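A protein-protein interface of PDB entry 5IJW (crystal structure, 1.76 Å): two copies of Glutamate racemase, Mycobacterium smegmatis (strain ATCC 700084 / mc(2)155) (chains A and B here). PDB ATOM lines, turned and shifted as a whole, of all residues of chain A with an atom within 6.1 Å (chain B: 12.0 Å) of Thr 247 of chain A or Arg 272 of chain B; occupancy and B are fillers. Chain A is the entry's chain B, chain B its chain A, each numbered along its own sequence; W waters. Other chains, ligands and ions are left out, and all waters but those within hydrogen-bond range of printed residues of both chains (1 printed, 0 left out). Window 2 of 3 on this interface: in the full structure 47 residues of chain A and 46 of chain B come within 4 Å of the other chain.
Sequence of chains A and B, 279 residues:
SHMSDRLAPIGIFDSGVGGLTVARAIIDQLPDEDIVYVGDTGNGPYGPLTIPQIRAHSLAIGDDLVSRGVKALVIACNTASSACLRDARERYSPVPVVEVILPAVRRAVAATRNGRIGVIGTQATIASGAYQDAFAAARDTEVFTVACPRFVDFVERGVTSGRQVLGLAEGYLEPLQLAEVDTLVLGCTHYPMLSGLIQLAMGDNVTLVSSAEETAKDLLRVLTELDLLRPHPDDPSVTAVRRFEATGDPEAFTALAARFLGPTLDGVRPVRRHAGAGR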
ATOM      1  N   SER A  15      -2.667 -12.466 -26.809  1.00  0.00           N
ATOM      2  CA  SER A  15      -3.933 -13.158 -26.613  1.00  0.00           C
ATOM      3  C   SER A  15      -3.748 -14.637 -26.321  1.00  0.00           C
ATOM      4  O   SER A  15      -4.663 -15.268 -25.776  1.00  0.00           O
ATOM      5  CB  SER A  15      -4.820 -12.996 -27.855  1.00  0.00           C
ATOM      6  OG  SER A  15      -4.281 -13.712 -28.953  1.00  0.00           O
ATOM      7  N   VAL A  38       3.216 -13.678 -21.084  1.00  0.00           N
ATOM      8  CA  VAL A  38       1.877 -14.088 -20.659  1.00  0.00           C
ATOM      9  C   VAL A  38       0.983 -14.238 -21.883  1.00  0.00           C
ATOM     10  O   VAL A  38       0.820 -13.289 -22.661  1.00  0.00           O
ATOM     11  CB  VAL A  38       1.243 -13.085 -19.677  1.00  0.00           C
ATOM     12  CG1 VAL A  38      -0.120 -13.616 -19.223  1.00  0.00           C
ATOM     13  CG2 VAL A  38       2.166 -12.855 -18.482  1.00  0.00           C
ATOM     14  N   GLY A  39       0.386 -15.417 -22.043  1.00  0.00           N
ATOM     15  CA  GLY A  39      -0.544 -15.677 -23.132  1.00  0.00           C
ATOM     16  C   GLY A  39      -1.938 -15.891 -22.565  1.00  0.00           C
ATOM     17  O   GLY A  39      -2.140 -16.750 -21.707  1.00  0.00           O
ATOM     18  N   ASP A  40      -2.887 -15.092 -23.045  1.00  0.00           N
ATOM     19  CA  ASP A  40      -4.242 -15.095 -22.473  1.00  0.00           C
ATOM     20  C   ASP A  40      -5.111 -16.209 -23.058  1.00  0.00           C
ATOM     21  O   ASP A  40      -6.226 -15.959 -23.509  1.00  0.00           O
ATOM     22  CB  ASP A  40      -4.896 -13.733 -22.677  1.00  0.00           C
ATOM     23  CG  ASP A  40      -6.083 -13.513 -21.747  1.00  0.00           C
ATOM     24  OD1 ASP A  40      -6.284 -14.350 -20.833  1.00  0.00           O
ATOM     25  OD2 ASP A  40      -6.806 -12.498 -21.916  1.00  0.00           O
ATOM     26  N   THR A  41      -4.607 -17.446 -23.050  1.00  0.00           N
ATOM     27  CA  THR A  41      -5.322 -18.551 -23.685  1.00  0.00           C
ATOM     28  C   THR A  41      -6.674 -18.811 -23.031  1.00  0.00           C
ATOM     29  O   THR A  41      -7.568 -19.372 -23.673  1.00  0.00           O
ATOM     30  CB  THR A  41      -4.485 -19.825 -23.641  1.00  0.00           C
ATOM     31  OG1 THR A  41      -4.074 -20.071 -22.291  1.00  0.00           O
ATOM     32  CG2 THR A  41      -3.240 -19.699 -24.533  1.00  0.00           C
ATOM     33  N   GLY A  42      -6.854 -18.396 -21.781  1.00  0.00           N
ATOM     34  CA  GLY A  42      -8.125 -18.638 -21.123  1.00  0.00           C
ATOM     35  C   GLY A  42      -9.247 -17.732 -21.579  1.00  0.00           C
ATOM     36  O   GLY A  42     -10.416 -18.042 -21.328  1.00  0.00           O
ATOM     37  N   ASN A  43      -8.923 -16.615 -22.237  1.00  0.00           N
ATOM     38  CA  ASN A  43      -9.938 -15.660 -22.658  1.00  0.00           C
ATOM     39  C   ASN A  43      -9.924 -15.345 -24.143  1.00  0.00           C
ATOM     40  O   ASN A  43     -10.893 -14.752 -24.633  1.00  0.00           O
ATOM     41  CB  ASN A  43      -9.794 -14.348 -21.879  1.00  0.00           C
ATOM     42  CG  ASN A  43      -9.969 -14.546 -20.395  1.00  0.00           C
ATOM     43  OD1 ASN A  43     -11.081 -14.814 -19.926  1.00  0.00           O
ATOM     44  ND2 ASN A  43      -8.881 -14.415 -19.642  1.00  0.00           N
ATOM     45  N   GLY A  44      -8.868 -15.696 -24.861  1.00  0.00           N
ATOM     46  CA  GLY A  44      -8.820 -15.476 -26.298  1.00  0.00           C
ATOM     47  C   GLY A  44      -9.517 -16.584 -27.070  1.00  0.00           C
ATOM     48  O   GLY A  44     -10.070 -17.514 -26.473  1.00  0.00           O
ATOM     49  N   ILE A  61      -3.813  -7.981 -18.039  1.00  0.00           N
ATOM     50  CA  ILE A  61      -2.499  -8.609 -18.079  1.00  0.00           C
ATOM     51  C   ILE A  61      -1.400  -7.552 -18.072  1.00  0.00           C
ATOM     52  O   ILE A  61      -0.423  -7.656 -17.320  1.00  0.00           O
ATOM     53  CB  ILE A  61      -2.402  -9.540 -19.299  1.00  0.00           C
ATOM     54  CG1 ILE A  61      -3.394 -10.690 -19.119  1.00  0.00           C
ATOM     55  CG2 ILE A  61      -0.976 -10.020 -19.481  1.00  0.00           C
ATOM     56  CD1 ILE A  61      -3.492 -11.635 -20.287  1.00  0.00           C
ATOM     57  N   PHE A 244       7.197 -18.400 -18.854  1.00  0.00           N
ATOM     58  CA  PHE A 244       6.034 -18.421 -19.731  1.00  0.00           C
ATOM     59  C   PHE A 244       4.795 -18.777 -18.920  1.00  0.00           C
ATOM     60  O   PHE A 244       4.788 -19.772 -18.184  1.00  0.00           O
ATOM     61  CB  PHE A 244       6.270 -19.396 -20.883  1.00  0.00           C
ATOM     62  CG  PHE A 244       7.442 -19.006 -21.754  1.00  0.00           C
ATOM     63  CD1 PHE A 244       8.741 -19.351 -21.394  1.00  0.00           C
ATOM     64  CD2 PHE A 244       7.246 -18.257 -22.909  1.00  0.00           C
ATOM     65  CE1 PHE A 244       9.820 -18.976 -22.190  1.00  0.00           C
ATOM     66  CE2 PHE A 244       8.316 -17.874 -23.695  1.00  0.00           C
ATOM     67  CZ  PHE A 244       9.607 -18.235 -23.333  1.00  0.00           C
ATOM     68  N   GLU A 245       3.761 -17.946 -19.037  1.00  0.00           N
ATOM     69  CA  GLU A 245       2.541 -18.078 -18.251  1.00  0.00           C
ATOM     70  C   GLU A 245       1.345 -18.167 -19.185  1.00  0.00           C
ATOM     71  O   GLU A 245       1.308 -17.498 -20.224  1.00  0.00           O
ATOM     72  CB  GLU A 245       2.365 -16.882 -17.289  1.00  0.00           C
ATOM     73  CG  GLU A 245       3.584 -16.619 -16.409  1.00  0.00           C
ATOM     74  CD  GLU A 245       3.370 -15.502 -15.416  1.00  0.00           C
ATOM     75  OE1 GLU A 245       2.302 -14.859 -15.457  1.00  0.00           O
ATOM     76  OE2 GLU A 245       4.277 -15.266 -14.589  1.00  0.00           O
ATOM     77  N   ALA A 246       0.366 -18.997 -18.815  1.00  0.00           N
ATOM     78  CA  ALA A 246      -0.878 -19.123 -19.559  1.00  0.00           C
ATOM     79  C   ALA A 246      -2.050 -18.865 -18.626  1.00  0.00           C
ATOM     80  O   ALA A 246      -2.039 -19.314 -17.478  1.00  0.00           O
ATOM     81  CB  ALA A 246      -1.020 -20.516 -20.180  1.00  0.00           C
ATOM     82  N   THR A 247      -3.058 -18.133 -19.112  1.00  0.00           N
ATOM     83  CA  THR A 247      -4.276 -17.984 -18.319  1.00  0.00           C
ATOM     84  C   THR A 247      -5.226 -19.162 -18.504  1.00  0.00           C
ATOM     85  O   THR A 247      -6.102 -19.371 -17.659  1.00  0.00           O
ATOM     86  CB  THR A 247      -4.998 -16.668 -18.649  1.00  0.00           C
ATOM     87  OG1 THR A 247      -5.441 -16.670 -20.015  1.00  0.00           O
ATOM     88  CG2 THR A 247      -4.066 -15.473 -18.410  1.00  0.00           C
ATOM     89  N   GLY A 248      -5.066 -19.938 -19.573  1.00  0.00           N
ATOM     90  CA  GLY A 248      -5.801 -21.164 -19.779  1.00  0.00           C
ATOM     91  C   GLY A 248      -4.985 -22.371 -19.366  1.00  0.00           C
ATOM     92  O   GLY A 248      -4.037 -22.271 -18.578  1.00  0.00           O
ATOM     93  N   ASP A 249      -5.354 -23.526 -19.906  1.00  0.00           N
ATOM     94  CA  ASP A 249      -4.686 -24.773 -19.530  1.00  0.00           C
ATOM     95  C   ASP A 249      -3.233 -24.758 -19.989  1.00  0.00           C
ATOM     96  O   ASP A 249      -2.978 -24.588 -21.191  1.00  0.00           O
ATOM     97  CB  ASP A 249      -5.402 -25.975 -20.132  1.00  0.00           C
ATOM     98  CG  ASP A 249      -4.638 -27.274 -19.910  1.00  0.00           C
ATOM     99  OD1 ASP A 249      -3.948 -27.397 -18.871  1.00  0.00           O
ATOM    100  OD2 ASP A 249      -4.715 -28.165 -20.779  1.00  0.00           O
ATOM    101  N   PRO A 250      -2.261 -24.919 -19.088  1.00  0.00           N
ATOM    102  CA  PRO A 250      -0.852 -24.910 -19.518  1.00  0.00           C
ATOM    103  C   PRO A 250      -0.478 -26.057 -20.443  1.00  0.00           C
ATOM    104  O   PRO A 250       0.436 -25.896 -21.263  1.00  0.00           O
ATOM    105  CB  PRO A 250      -0.085 -24.989 -18.193  1.00  0.00           C
ATOM    106  CG  PRO A 250      -1.031 -24.411 -17.179  1.00  0.00           C
ATOM    107  CD  PRO A 250      -2.392 -24.857 -17.621  1.00  0.00           C
ATOM    108  N   VAL B 268      10.921 -25.142 -22.067  1.00  0.00           N
ATOM    109  CA  VAL B 268       9.785 -24.299 -21.712  1.00  0.00           C
ATOM    110  C   VAL B 268       8.756 -25.129 -20.952  1.00  0.00           C
ATOM    111  O   VAL B 268       8.389 -26.235 -21.371  1.00  0.00           O
ATOM    112  CB  VAL B 268       9.185 -23.652 -22.971  1.00  0.00           C
ATOM    113  CG1 VAL B 268       7.968 -22.816 -22.629  1.00  0.00           C
ATOM    114  CG2 VAL B 268      10.229 -22.792 -23.663  1.00  0.00           C
ATOM    115  N   ARG B 269       8.313 -24.609 -19.808  1.00  0.00           N
ATOM    116  CA  ARG B 269       7.282 -25.247 -18.990  1.00  0.00           C
ATOM    117  C   ARG B 269       6.375 -24.145 -18.454  1.00  0.00           C
ATOM    118  O   ARG B 269       6.736 -23.452 -17.488  1.00  0.00           O
ATOM    119  CB  ARG B 269       7.892 -26.065 -17.853  1.00  0.00           C
ATOM    120  N   PRO B 270       5.203 -23.943 -19.060  1.00  0.00           N
ATOM    121  CA  PRO B 270       4.362 -22.798 -18.688  1.00  0.00           C
ATOM    122  C   PRO B 270       3.688 -22.977 -17.340  1.00  0.00           C
ATOM    123  O   PRO B 270       3.333 -24.085 -16.933  1.00  0.00           O
ATOM    124  CB  PRO B 270       3.318 -22.738 -19.814  1.00  0.00           C
ATOM    125  CG  PRO B 270       3.245 -24.132 -20.315  1.00  0.00           C
ATOM    126  CD  PRO B 270       4.644 -24.682 -20.203  1.00  0.00           C
ATOM    127  N   VAL B 271       3.494 -21.864 -16.654  1.00  0.00           N
ATOM    128  CA  VAL B 271       2.822 -21.872 -15.362  1.00  0.00           C
ATOM    129  C   VAL B 271       1.450 -21.235 -15.517  1.00  0.00           C
ATOM    130  O   VAL B 271       1.160 -20.536 -16.491  1.00  0.00           O
ATOM    131  CB  VAL B 271       3.630 -21.147 -14.267  1.00  0.00           C
ATOM    132  CG1 VAL B 271       5.082 -21.625 -14.250  1.00  0.00           C
ATOM    133  CG2 VAL B 271       3.568 -19.653 -14.464  1.00  0.00           C
ATOM    134  N   ARG B 272       0.597 -21.477 -14.532  1.00  0.00           N
ATOM    135  CA  ARG B 272      -0.684 -20.786 -14.464  1.00  0.00           C
ATOM    136  C   ARG B 272      -0.800 -20.029 -13.144  1.00  0.00           C
ATOM    137  O   ARG B 272      -0.611 -20.618 -12.074  1.00  0.00           O
ATOM    138  CB  ARG B 272      -1.846 -21.762 -14.610  1.00  0.00           C
ATOM    139  CG  ARG B 272      -3.182 -21.158 -14.198  1.00  0.00           C
ATOM    140  CD  ARG B 272      -4.322 -21.653 -15.063  1.00  0.00           C
ATOM    141  NE  ARG B 272      -4.519 -23.094 -14.949  1.00  0.00           N
ATOM    142  CZ  ARG B 272      -5.500 -23.758 -15.552  1.00  0.00           C
ATOM    143  NH1 ARG B 272      -6.382 -23.103 -16.301  1.00  0.00           N
ATOM    144  NH2 ARG B 272      -5.603 -25.072 -15.410  1.00  0.00           N
HETATM  145  O   HOH W   1       8.071 -20.854 -17.685  1.00  0.00           O
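No position is printed for both chains. Of the 11 pairs that touch across the chains among the printed residues, none has its exchanged pair printed and touching as well.
Of the 5 printed residues of chain B, 4 touch a printed residue of chain A. Hydrophobic or aromatic side chains of chain B within 4 Å of the printed part of chain A: Val 268, Pro 270 and Val 271. Along chain B the printed residues that touch a printed residue of chain A span positions 268 to 272. Of the 16 printed residues of chain A, 7 touch a printed residue of chain B. Along chain A the printed residues that touch a printed residue of chain B span positions 244 to 250. Among the printed residues, no Asp or Glu carboxylate lies within 4 Å of a Lys or Arg side-chain nitrogen of the other chain.
O of Phe 244 of chain A is in hydrogen-bond range of N of Val 271 of chain B. The backbone NH (N) of Ala 246 of chain A lies within hydrogen-bond range of the backbone carbonyl oxygen (O) of Val 271 of chain B, 2.9 Å away. The backbone carbonyl oxygen of Gly 248 of chain A sits at hydrogen-bond distance from the guanidinium group of Arg 272 of chain B, 3.4 Å away.
Of chain B, only Arg 272 (3.9 Å) comes within 4 Å of Thr 247 of chain A. Of chain A, only Ala 246 (3.6 Å), Thr 247 (3.9 Å), Gly 248 (3.4 Å), Asp 249 (3.8 Å) and Pro 250 (3.8 Å) come within 4 Å of Arg 272 of chain B. No residue of chain B comes within 4 Å of Gly 39 of chain A. Asp 40 of chain A touches none of the printed residues of chain B. No residue of chain B comes within 4 Å of Thr 41 of chain A. No residue of chain B comes within 4 Å of Asn 43 of chain A. Glu 245 of chain A touches just one residue of chain B: Val 271. Ala 246 of chain A touches just these residues of chain B: Val 271 and Arg 272. Printed residues of chain B within 4 Å of Gly 248 of chain A: Arg 272 (3.4 Å). Asp 249 of chain A touches just one residue of chain B: Arg 272 (3.8 Å). Of the printed residues of chain A, Val 268 of chain B touches Phe 244 (3.8 Å). Printed residues of chain B within 4 Å of Pro 250 of chain A: Pro 270 and Arg 272. Of the printed residues of chain A, Pro 270 of chain B touches Phe 244 (3.1 Å) and Pro 250 (3.4 Å). Printed residues of chain A within 4 Å of Val 271 of chain B: Phe 244 (2.9 Å), Glu 245 (3.3 Å) and Ala 246 (2.9 Å). Printed residues of chain B within 4 Å of Phe 244 of chain A: Val 268 (3.8 Å), Pro 270 (3.1 Å) and Val 271 (2.9 Å). Ile 61 of chain A touches none of the printed residues of chain B. Gly 44 of chain A touches none of the printed residues of chain B. The nearest residue of chain A that does not touch Arg 272 of chain B is Glu 245 of chain A (5.4 Å).
Among the printed residues, merely in contact across the chains: Phe 244 of chain A with Val 268 of chain B (3.8 Å), Phe 244 of chain A with Pro 270 of chain B (3.1 Å), Glu 245 of chain A with Val 271 of chain B (3.3 Å), Ala 246 of chain A with Arg 272 of chain B (3.6 Å), Thr 247 of chain A with Arg 272 of chain B (3.9 Å), Asp 249 of chain A with Arg 272 of chain B (3.8 Å), Pro 250 of chain A with Pro 270 of chain B (3.4 Å) and Pro 250 of chain A with Arg 272 of chain B (3.8 Å).
The backbone NH (N) of Gly 39 of chain A lies within hydrogen-bond range of the backbone carbonyl oxygen (O) of Glu 245 of chain A (2.9 Å). N of Thr 247 of chain A sits at hydrogen-bond distance from O of Gly 39 of chain A, at 3.1 Å. OD1 of Asp 40 of chain A is in hydrogen-bond range of OG1 of Thr 247 of chain A (2.6 Å). OG1 of Thr 247 of chain A sits at hydrogen-bond distance from N of Thr 41 of chain A, 3.2 Å away. The side-chain hydroxyl (OG1) of Thr 41 of chain A is in hydrogen-bond range of the backbone NH (N) of Gly 248 of chain A, 2.9 Å away. OG1 of Thr 247 of chain A sits at hydrogen-bond distance from N of Gly 42 of chain A (2.8 Å).
Water W1 lies within hydrogen-bond range of the backbone NH (N) of Phe 244 of chain A (2.9 Å) and the backbone carbonyl oxygen (O) of Arg 269 of chain B (2.9 Å).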
